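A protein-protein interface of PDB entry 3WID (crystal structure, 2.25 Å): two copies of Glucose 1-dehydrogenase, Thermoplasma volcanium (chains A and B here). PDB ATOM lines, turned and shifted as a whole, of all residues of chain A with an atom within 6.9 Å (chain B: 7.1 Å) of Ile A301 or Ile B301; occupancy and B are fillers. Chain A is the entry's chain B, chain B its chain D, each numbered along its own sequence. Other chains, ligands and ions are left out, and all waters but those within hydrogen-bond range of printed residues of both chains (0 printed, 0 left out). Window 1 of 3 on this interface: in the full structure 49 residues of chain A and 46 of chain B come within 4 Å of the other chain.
Val A171 touches its own counterpart, Val B171.
Ile A299 touches Gly B303, and with the chains exchanged Gly A303 touches Ile B299.
Thr A300 touches Ile B301, and with the chains exchanged Ile A301 touches Thr B300.
Ile B301 touches its own counterpart, Ile A301.
16 positions are printed for both chains.
Ile A301 touches two residues of chain B.
Of chain A, only Thr A300 (3.5 Å) and Ile A301 (2.7 Å) come within 4 Å of Ile B301.
Printed residues of chain B within 4 Å of Ile A299: Ala B302 and Gly B303.
Printed residues of chain B within 4 Å of Thr A300: Thr B300 (3.6 Å) and Ile B301 (3.5 Å).
The nearest residue of chain A that does not touch Ile B301 is Ile A299 (4.2 Å).
NH2 of Arg A174 sits at hydrogen-bond distance from O of Gly B303 (2.5 Å).
O of Ile A299 is in hydrogen-bond range of N of Gly B303 (3.0 Å).
N of Ile A301 lies within hydrogen-bond range of O of Ile B301 (2.7 Å).
The backbone carbonyl oxygen of Gly A303 is in hydrogen-bond range of the guanidinium group of Arg B174 (2.6 Å).
The backbone NH (N) of Gly A303 sits at hydrogen-bond distance from the backbone carbonyl oxygen (O) of Ile B299 (2.9 Å).
Among the printed residues, merely in contact across the chains: Val A171 with Val B171 (3.99 Å), Arg A174 with Ala B302 (3.6 Å), Ile A294 with Leu B274 (3.9 Å), Ile A299 with Ala B302 (3.8 Å), Thr A300 with Thr B300 (3.6 Å), Thr A300 with Ile B301 (3.5 Å), Ile A301 with Thr B300 (3.6 Å), Ala A302 with Arg B174 (3.5 Å) and Ala A302 with Ile B299 (3.6 Å).
The guanidinium group of Arg A174 sits at hydrogen-bond distance from the side-chain hydroxyl of Thr A300, at 2.9 Å.
The backbone carbonyl oxygen (O) of Val A272 is in hydrogen-bond range of the backbone NH (N) of Ala A302 (2.9 Å).
The backbone NH of Thr B300 lies within hydrogen-bond range of the backbone carbonyl oxygen of Gly B270, 3.1 Å away.
The backbone NH (N) of Val B272 sits at hydrogen-bond distance from the backbone carbonyl oxygen (O) of Thr B300 (2.7 Å).
The backbone carbonyl oxygen (O) of Val B272 sits at hydrogen-bond distance from the backbone NH (N) of Ala B302 (2.8 Å).
The backbone carbonyl oxygen (O) of Ile B294 sits at hydrogen-bond distance from the backbone NH (N) of Ile B299, 3.2 Å away.
Printed residues of chain B that touch a printed residue of chain A: Val B171, Arg B174, Leu B274, Ile B299, Thr B300, Ile B301, Ala B302 and Gly B303.
Hydrophobic or aromatic side chains of chain B that line the printed part of chain A: Val B171, Leu B274, Ile B301 and Ala B302.
Of the 16 printed residues of chain A, 8 touch a printed residue of chain B.
Among the printed residues, no Asp or Glu carboxylate lies within 4 Å of a Lys or Arg side-chain nitrogen of the other chain.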
ATOM      1  N   VAL A 171     -13.982  38.934   6.277  1.00  0.00           N
ATOM      2  CA  VAL A 171     -12.798  38.089   6.053  1.00  0.00           C
ATOM      3  C   VAL A 171     -11.600  38.956   5.738  1.00  0.00           C
ATOM      4  O   VAL A 171     -10.480  38.612   6.063  1.00  0.00           O
ATOM      5  CB  VAL A 171     -13.014  36.925   5.041  1.00  0.00           C
ATOM      6  CG1 VAL A 171     -14.208  36.015   5.447  1.00  0.00           C
ATOM      7  CG2 VAL A 171     -13.188  37.426   3.613  1.00  0.00           C
ATOM      8  N   ARG A 174      -8.590  40.183   8.189  1.00  0.00           N
ATOM      9  CA  ARG A 174      -7.444  39.389   8.531  1.00  0.00           C
ATOM     10  C   ARG A 174      -6.116  40.125   8.361  1.00  0.00           C
ATOM     11  O   ARG A 174      -5.194  39.856   9.039  1.00  0.00           O
ATOM     12  CB  ARG A 174      -7.496  37.994   7.933  1.00  0.00           C
ATOM     13  CG  ARG A 174      -7.118  37.841   6.500  1.00  0.00           C
ATOM     14  CD  ARG A 174      -7.352  36.413   6.112  1.00  0.00           C
ATOM     15  NE  ARG A 174      -6.110  35.707   6.189  1.00  0.00           N
ATOM     16  CZ  ARG A 174      -5.849  34.550   5.644  1.00  0.00           C
ATOM     17  NH1 ARG A 174      -6.743  33.901   4.973  1.00  0.00           N
ATOM     18  NH2 ARG A 174      -4.663  34.042   5.780  1.00  0.00           N
ATOM     19  N   ILE A 259     -12.931  29.211 -12.391  1.00  0.00           N
ATOM     20  CA  ILE A 259     -12.639  29.680 -11.021  1.00  0.00           C
ATOM     21  C   ILE A 259     -11.171  29.582 -10.665  1.00  0.00           C
ATOM     22  O   ILE A 259     -10.514  30.574 -10.295  1.00  0.00           O
ATOM     23  CB  ILE A 259     -13.444  28.871 -10.003  1.00  0.00           C
ATOM     24  CG1 ILE A 259     -14.946  29.245 -10.092  1.00  0.00           C
ATOM     25  CG2 ILE A 259     -12.961  29.155  -8.619  1.00  0.00           C
ATOM     26  CD1 ILE A 259     -15.829  28.328  -9.303  1.00  0.00           C
ATOM     27  N   PHE A 260     -10.641  28.359 -10.742  1.00  0.00           N
ATOM     28  CA  PHE A 260      -9.245  28.152 -10.346  1.00  0.00           C
ATOM     29  C   PHE A 260      -8.232  28.848 -11.253  1.00  0.00           C
ATOM     30  O   PHE A 260      -7.197  29.345 -10.766  1.00  0.00           O
ATOM     31  CB  PHE A 260      -8.959  26.704 -10.118  1.00  0.00           C
ATOM     32  CG  PHE A 260      -9.554  26.193  -8.880  1.00  0.00           C
ATOM     33  CD1 PHE A 260      -8.996  26.513  -7.653  1.00  0.00           C
ATOM     34  CD2 PHE A 260     -10.731  25.461  -8.912  1.00  0.00           C
ATOM     35  CE1 PHE A 260      -9.590  26.067  -6.466  1.00  0.00           C
ATOM     36  CE2 PHE A 260     -11.327  25.024  -7.758  1.00  0.00           C
ATOM     37  CZ  PHE A 260     -10.743  25.304  -6.533  1.00  0.00           C
ATOM     38  N   VAL A 263      -8.200  32.213  -9.745  1.00  0.00           N
ATOM     39  CA  VAL A 263      -7.538  32.159  -8.437  1.00  0.00           C
ATOM     40  C   VAL A 263      -6.027  32.377  -8.542  1.00  0.00           C
ATOM     41  O   VAL A 263      -5.453  33.071  -7.692  1.00  0.00           O
ATOM     42  CB  VAL A 263      -7.901  30.865  -7.667  1.00  0.00           C
ATOM     43  CG1 VAL A 263      -7.026  30.683  -6.421  1.00  0.00           C
ATOM     44  CG2 VAL A 263      -9.391  30.892  -7.247  1.00  0.00           C
ATOM     45  N   GLY A 270      -5.835  38.575  -1.057  1.00  0.00           N
ATOM     46  CA  GLY A 270      -6.922  38.631  -1.983  1.00  0.00           C
ATOM     47  C   GLY A 270      -8.049  37.818  -1.493  1.00  0.00           C
ATOM     48  O   GLY A 270      -7.857  36.965  -0.616  1.00  0.00           O
ATOM     49  N   VAL A 271      -9.255  38.186  -1.952  1.00  0.00           N
ATOM     50  CA  VAL A 271     -10.417  37.466  -1.542  1.00  0.00           C
ATOM     51  C   VAL A 271     -11.182  36.934  -2.712  1.00  0.00           C
ATOM     52  O   VAL A 271     -11.384  37.615  -3.693  1.00  0.00           O
ATOM     53  CB  VAL A 271     -11.345  38.321  -0.667  1.00  0.00           C
ATOM     54  CG1 VAL A 271     -12.594  37.519  -0.342  1.00  0.00           C
ATOM     55  CG2 VAL A 271     -10.606  38.803   0.547  1.00  0.00           C
ATOM     56  N   VAL A 272     -11.622  35.709  -2.583  1.00  0.00           N
ATOM     57  CA  VAL A 272     -12.422  35.092  -3.648  1.00  0.00           C
ATOM     58  C   VAL A 272     -13.758  34.748  -3.074  1.00  0.00           C
ATOM     59  O   VAL A 272     -13.796  34.090  -2.031  1.00  0.00           O
ATOM     60  CB  VAL A 272     -11.760  33.796  -4.141  1.00  0.00           C
ATOM     61  CG1 VAL A 272     -12.610  33.064  -5.143  1.00  0.00           C
ATOM     62  CG2 VAL A 272     -10.365  34.133  -4.677  1.00  0.00           C
ATOM     63  N   ILE A 273     -14.837  35.143  -3.781  1.00  0.00           N
ATOM     64  CA  ILE A 273     -16.187  34.823  -3.350  1.00  0.00           C
ATOM     65  C   ILE A 273     -16.710  33.791  -4.326  1.00  0.00           C
ATOM     66  O   ILE A 273     -16.845  34.037  -5.550  1.00  0.00           O
ATOM     67  CB  ILE A 273     -17.129  36.058  -3.289  1.00  0.00           C
ATOM     68  CG1 ILE A 273     -16.654  37.131  -2.318  1.00  0.00           C
ATOM     69  CG2 ILE A 273     -18.544  35.667  -2.939  1.00  0.00           C
ATOM     70  CD1 ILE A 273     -16.645  36.670  -0.904  1.00  0.00           C
ATOM     71  N   LEU A 274     -17.073  32.652  -3.765  1.00  0.00           N
ATOM     72  CA  LEU A 274     -17.757  31.663  -4.544  1.00  0.00           C
ATOM     73  C   LEU A 274     -19.252  31.895  -4.366  1.00  0.00           C
ATOM     74  O   LEU A 274     -19.729  31.934  -3.261  1.00  0.00           O
ATOM     75  CB  LEU A 274     -17.349  30.244  -4.134  1.00  0.00           C
ATOM     76  CG  LEU A 274     -15.899  29.880  -4.432  1.00  0.00           C
ATOM     77  CD1 LEU A 274     -15.562  28.470  -4.000  1.00  0.00           C
ATOM     78  CD2 LEU A 274     -15.529  30.053  -5.906  1.00  0.00           C
ATOM     79  N   ILE A 294      -2.308  29.564  -2.886  1.00  0.00           N
ATOM     80  CA  ILE A 294      -3.341  30.080  -1.957  1.00  0.00           C
ATOM     81  C   ILE A 294      -2.755  30.260  -0.583  1.00  0.00           C
ATOM     82  O   ILE A 294      -2.856  31.309   0.036  1.00  0.00           O
ATOM     83  CB  ILE A 294      -4.510  29.115  -1.926  1.00  0.00           C
ATOM     84  CG1 ILE A 294      -5.122  29.113  -3.315  1.00  0.00           C
ATOM     85  CG2 ILE A 294      -5.498  29.481  -0.831  1.00  0.00           C
ATOM     86  CD1 ILE A 294      -6.152  28.031  -3.547  1.00  0.00           C
ATOM     87  N   ILE A 299      -4.681  33.952   0.945  1.00  0.00           N
ATOM     88  CA  ILE A 299      -5.902  34.168   0.211  1.00  0.00           C
ATOM     89  C   ILE A 299      -7.026  33.516   0.964  1.00  0.00           C
ATOM     90  O   ILE A 299      -6.828  32.528   1.680  1.00  0.00           O
ATOM     91  CB  ILE A 299      -5.777  33.576  -1.174  1.00  0.00           C
ATOM     92  CG1 ILE A 299      -5.040  34.569  -2.050  1.00  0.00           C
ATOM     93  CG2 ILE A 299      -7.114  33.223  -1.813  1.00  0.00           C
ATOM     94  CD1 ILE A 299      -4.498  33.934  -3.335  1.00  0.00           C
ATOM     95  N   THR A 300      -8.236  34.026   0.760  1.00  0.00           N
ATOM     96  CA  THR A 300      -9.394  33.458   1.430  1.00  0.00           C
ATOM     97  C   THR A 300     -10.405  33.201   0.368  1.00  0.00           C
ATOM     98  O   THR A 300     -10.614  34.053  -0.535  1.00  0.00           O
ATOM     99  CB  THR A 300     -10.012  34.464   2.426  1.00  0.00           C
ATOM    100  OG1 THR A 300      -9.096  34.801   3.456  1.00  0.00           O
ATOM    101  CG2 THR A 300     -11.228  33.906   3.044  1.00  0.00           C
ATOM    102  N   ILE A 301     -11.033  32.036   0.439  1.00  0.00           N
ATOM    103  CA  ILE A 301     -12.021  31.644  -0.567  1.00  0.00           C
ATOM    104  C   ILE A 301     -13.267  31.353   0.218  1.00  0.00           C
ATOM    105  O   ILE A 301     -13.315  30.350   0.945  1.00  0.00           O
ATOM    106  CB  ILE A 301     -11.605  30.349  -1.291  1.00  0.00           C
ATOM    107  CG1 ILE A 301     -10.317  30.604  -2.051  1.00  0.00           C
ATOM    108  CG2 ILE A 301     -12.699  29.845  -2.216  1.00  0.00           C
ATOM    109  CD1 ILE A 301      -9.647  29.355  -2.592  1.00  0.00           C
ATOM    110  N   ALA A 302     -14.271  32.206   0.061  1.00  0.00           N
ATOM    111  CA  ALA A 302     -15.492  32.095   0.842  1.00  0.00           C
ATOM    112  C   ALA A 302     -16.747  31.875  -0.035  1.00  0.00           C
ATOM    113  O   ALA A 302     -17.045  32.618  -0.938  1.00  0.00           O
ATOM    114  CB  ALA A 302     -15.612  33.344   1.708  1.00  0.00           C
ATOM    115  N   GLY A 303     -17.464  30.815   0.227  1.00  0.00           N
ATOM    116  CA  GLY A 303     -18.745  30.597  -0.387  1.00  0.00           C
ATOM    117  C   GLY A 303     -19.802  31.369   0.373  1.00  0.00           C
ATOM    118  O   GLY A 303     -19.730  31.522   1.608  1.00  0.00           O
ATOM    119  N   VAL B 171     -12.255  35.076  10.310  1.00  0.00           N
ATOM    120  CA  VAL B 171     -13.203  34.612   9.276  1.00  0.00           C
ATOM    121  C   VAL B 171     -14.437  33.959   9.843  1.00  0.00           C
ATOM    122  O   VAL B 171     -15.536  34.029   9.244  1.00  0.00           O
ATOM    123  CB  VAL B 171     -12.578  33.666   8.232  1.00  0.00           C
ATOM    124  CG1 VAL B 171     -11.348  34.301   7.641  1.00  0.00           C
ATOM    125  CG2 VAL B 171     -12.293  32.265   8.812  1.00  0.00           C
ATOM    126  N   ARG B 174     -17.999  35.570  10.380  1.00  0.00           N
ATOM    127  CA  ARG B 174     -19.056  35.788   9.395  1.00  0.00           C
ATOM    128  C   ARG B 174     -20.446  35.295   9.865  1.00  0.00           C
ATOM    129  O   ARG B 174     -21.453  35.623   9.281  1.00  0.00           O
ATOM    130  CB  ARG B 174     -18.693  35.249   8.005  1.00  0.00           C
ATOM    131  CG  ARG B 174     -18.460  33.787   7.921  1.00  0.00           C
ATOM    132  CD  ARG B 174     -17.921  33.382   6.538  1.00  0.00           C
ATOM    133  NE  ARG B 174     -19.045  33.373   5.607  1.00  0.00           N
ATOM    134  CZ  ARG B 174     -19.091  32.786   4.445  1.00  0.00           C
ATOM    135  NH1 ARG B 174     -18.032  32.101   3.955  1.00  0.00           N
ATOM    136  NH2 ARG B 174     -20.219  32.859   3.772  1.00  0.00           N
ATOM    137  N   ILE B 259      -7.405  16.953   0.855  1.00  0.00           N
ATOM    138  CA  ILE B 259      -8.059  18.199   1.163  1.00  0.00           C
ATOM    139  C   ILE B 259      -9.551  18.184   0.790  1.00  0.00           C
ATOM    140  O   ILE B 259     -10.424  18.331   1.688  1.00  0.00           O
ATOM    141  CB  ILE B 259      -7.347  19.389   0.511  1.00  0.00           C
ATOM    142  CG1 ILE B 259      -6.032  19.615   1.216  1.00  0.00           C
ATOM    143  CG2 ILE B 259      -8.182  20.661   0.636  1.00  0.00           C
ATOM    144  CD1 ILE B 259      -5.054  20.506   0.479  1.00  0.00           C
ATOM    145  N   PHE B 260      -9.812  18.058  -0.507  1.00  0.00           N
ATOM    146  CA  PHE B 260     -11.141  18.192  -1.047  1.00  0.00           C
ATOM    147  C   PHE B 260     -12.056  17.066  -0.640  1.00  0.00           C
ATOM    148  O   PHE B 260     -13.288  17.255  -0.662  1.00  0.00           O
ATOM    149  CB  PHE B 260     -11.159  18.369  -2.563  1.00  0.00           C
ATOM    150  CG  PHE B 260     -10.786  19.733  -2.968  1.00  0.00           C
ATOM    151  CD1 PHE B 260     -11.706  20.779  -2.838  1.00  0.00           C
ATOM    152  CD2 PHE B 260      -9.492  20.029  -3.349  1.00  0.00           C
ATOM    153  CE1 PHE B 260     -11.345  22.070  -3.134  1.00  0.00           C
ATOM    154  CE2 PHE B 260      -9.125  21.324  -3.637  1.00  0.00           C
ATOM    155  CZ  PHE B 260     -10.053  22.347  -3.530  1.00  0.00           C
ATOM    156  N   VAL B 263     -13.176  18.304   2.805  1.00  0.00           N
ATOM    157  CA  VAL B 263     -14.017  19.505   2.652  1.00  0.00           C
ATOM    158  C   VAL B 263     -15.466  19.067   2.525  1.00  0.00           C
ATOM    159  O   VAL B 263     -16.343  19.688   3.121  1.00  0.00           O
ATOM    160  CB  VAL B 263     -13.611  20.366   1.426  1.00  0.00           C
ATOM    161  CG1 VAL B 263     -14.682  21.364   1.097  1.00  0.00           C
ATOM    162  CG2 VAL B 263     -12.339  21.169   1.687  1.00  0.00           C
ATOM    163  N   GLY B 270     -18.637  25.942   8.300  1.00  0.00           N
ATOM    164  CA  GLY B 270     -17.297  25.386   8.566  1.00  0.00           C
ATOM    165  C   GLY B 270     -16.197  26.214   7.965  1.00  0.00           C
ATOM    166  O   GLY B 270     -16.391  26.935   6.998  1.00  0.00           O
ATOM    167  N   VAL B 271     -15.053  26.148   8.618  1.00  0.00           N
ATOM    168  CA  VAL B 271     -13.830  26.772   8.173  1.00  0.00           C
ATOM    169  C   VAL B 271     -12.742  25.746   7.802  1.00  0.00           C
ATOM    170  O   VAL B 271     -12.496  24.768   8.523  1.00  0.00           O
ATOM    171  CB  VAL B 271     -13.269  27.698   9.306  1.00  0.00           C
ATOM    172  CG1 VAL B 271     -11.896  28.261   8.962  1.00  0.00           C
ATOM    173  CG2 VAL B 271     -14.244  28.849   9.591  1.00  0.00           C
ATOM    174  N   VAL B 272     -12.065  25.995   6.700  1.00  0.00           N
ATOM    175  CA  VAL B 272     -11.031  25.078   6.206  1.00  0.00           C
ATOM    176  C   VAL B 272      -9.783  25.954   6.177  1.00  0.00           C
ATOM    177  O   VAL B 272      -9.799  26.975   5.485  1.00  0.00           O
ATOM    178  CB  VAL B 272     -11.347  24.559   4.773  1.00  0.00           C
ATOM    179  CG1 VAL B 272     -10.150  23.789   4.204  1.00  0.00           C
ATOM    180  CG2 VAL B 272     -12.546  23.636   4.734  1.00  0.00           C
ATOM    181  N   ILE B 273      -8.763  25.607   6.978  1.00  0.00           N
ATOM    182  CA  ILE B 273      -7.451  26.269   6.987  1.00  0.00           C
ATOM    183  C   ILE B 273      -6.480  25.479   6.087  1.00  0.00           C
ATOM    184  O   ILE B 273      -6.223  24.314   6.344  1.00  0.00           O
ATOM    185  CB  ILE B 273      -6.852  26.305   8.407  1.00  0.00           C
ATOM    186  CG1 ILE B 273      -7.730  27.125   9.364  1.00  0.00           C
ATOM    187  CG2 ILE B 273      -5.440  26.866   8.425  1.00  0.00           C
ATOM    188  CD1 ILE B 273      -7.889  28.567   8.947  1.00  0.00           C
ATOM    189  N   LEU B 274      -5.922  26.118   5.079  1.00  0.00           N
ATOM    190  CA  LEU B 274      -4.928  25.503   4.242  1.00  0.00           C
ATOM    191  C   LEU B 274      -3.581  26.000   4.751  1.00  0.00           C
ATOM    192  O   LEU B 274      -3.377  27.175   4.885  1.00  0.00           O
ATOM    193  CB  LEU B 274      -5.138  25.852   2.765  1.00  0.00           C
ATOM    194  CG  LEU B 274      -6.421  25.529   1.992  1.00  0.00           C
ATOM    195  CD1 LEU B 274      -6.365  25.943   0.541  1.00  0.00           C
ATOM    196  CD2 LEU B 274      -6.846  24.099   2.123  1.00  0.00           C
ATOM    197  N   ILE B 291     -17.955  22.726  -5.537  1.00  0.00           N
ATOM    198  CA  ILE B 291     -18.071  24.153  -5.373  1.00  0.00           C
ATOM    199  C   ILE B 291     -19.427  24.444  -4.740  1.00  0.00           C
ATOM    200  O   ILE B 291     -19.535  25.223  -3.771  1.00  0.00           O
ATOM    201  CB  ILE B 291     -17.991  24.824  -6.769  1.00  0.00           C
ATOM    202  CG1 ILE B 291     -16.604  24.605  -7.380  1.00  0.00           C
ATOM    203  CG2 ILE B 291     -18.326  26.309  -6.716  1.00  0.00           C
ATOM    204  CD1 ILE B 291     -15.474  25.317  -6.669  1.00  0.00           C
ATOM    205  N   ILE B 294     -19.514  23.995  -1.187  1.00  0.00           N
ATOM    206  CA  ILE B 294     -18.896  25.107  -0.462  1.00  0.00           C
ATOM    207  C   ILE B 294     -19.834  26.287  -0.370  1.00  0.00           C
ATOM    208  O   ILE B 294     -20.095  26.798   0.721  1.00  0.00           O
ATOM    209  CB  ILE B 294     -17.566  25.480  -1.111  1.00  0.00           C
ATOM    210  CG1 ILE B 294     -16.619  24.268  -0.994  1.00  0.00           C
ATOM    211  CG2 ILE B 294     -16.931  26.704  -0.459  1.00  0.00           C
ATOM    212  CD1 ILE B 294     -15.389  24.391  -1.834  1.00  0.00           C
ATOM    213  N   ILE B 299     -19.126  27.865   3.613  1.00  0.00           N
ATOM    214  CA  ILE B 299     -17.777  27.488   4.069  1.00  0.00           C
ATOM    215  C   ILE B 299     -16.748  28.558   3.670  1.00  0.00           C
ATOM    216  O   ILE B 299     -16.840  29.219   2.621  1.00  0.00           O
ATOM    217  CB  ILE B 299     -17.426  26.077   3.517  1.00  0.00           C
ATOM    218  CG1 ILE B 299     -18.392  25.054   4.140  1.00  0.00           C
ATOM    219  CG2 ILE B 299     -15.946  25.694   3.772  1.00  0.00           C
ATOM    220  CD1 ILE B 299     -18.214  23.639   3.599  1.00  0.00           C
ATOM    221  N   THR B 300     -15.743  28.718   4.522  1.00  0.00           N
ATOM    222  CA  THR B 300     -14.605  29.584   4.246  1.00  0.00           C
ATOM    223  C   THR B 300     -13.327  28.725   4.180  1.00  0.00           C
ATOM    224  O   THR B 300     -13.065  27.922   5.085  1.00  0.00           O
ATOM    225  CB  THR B 300     -14.441  30.633   5.325  1.00  0.00           C
ATOM    226  OG1 THR B 300     -15.722  31.314   5.546  1.00  0.00           O
ATOM    227  CG2 THR B 300     -13.320  31.647   4.878  1.00  0.00           C
ATOM    228  N   ILE B 301     -12.613  28.827   3.061  1.00  0.00           N
ATOM    229  CA  ILE B 301     -11.345  28.175   2.857  1.00  0.00           C
ATOM    230  C   ILE B 301     -10.257  29.252   2.888  1.00  0.00           C
ATOM    231  O   ILE B 301     -10.149  30.049   1.975  1.00  0.00           O
ATOM    232  CB  ILE B 301     -11.291  27.446   1.520  1.00  0.00           C
ATOM    233  CG1 ILE B 301     -12.359  26.331   1.468  1.00  0.00           C
ATOM    234  CG2 ILE B 301      -9.904  26.796   1.330  1.00  0.00           C
ATOM    235  CD1 ILE B 301     -12.586  25.771   0.070  1.00  0.00           C
ATOM    236  N   ALA B 302      -9.438  29.218   3.927  1.00  0.00           N
ATOM    237  CA  ALA B 302      -8.456  30.199   4.152  1.00  0.00           C
ATOM    238  C   ALA B 302      -7.016  29.623   4.207  1.00  0.00           C
ATOM    239  O   ALA B 302      -6.724  28.745   5.014  1.00  0.00           O
ATOM    240  CB  ALA B 302      -8.786  30.919   5.439  1.00  0.00           C
ATOM    241  N   GLY B 303      -6.172  30.100   3.295  1.00  0.00           N
ATOM    242  CA  GLY B 303      -4.742  29.871   3.311  1.00  0.00           C
ATOM    243  C   GLY B 303      -4.047  30.750   4.349  1.00  0.00           C
ATOM    244  O   GLY B 303      -4.353  31.942   4.433  1.00  0.00           O
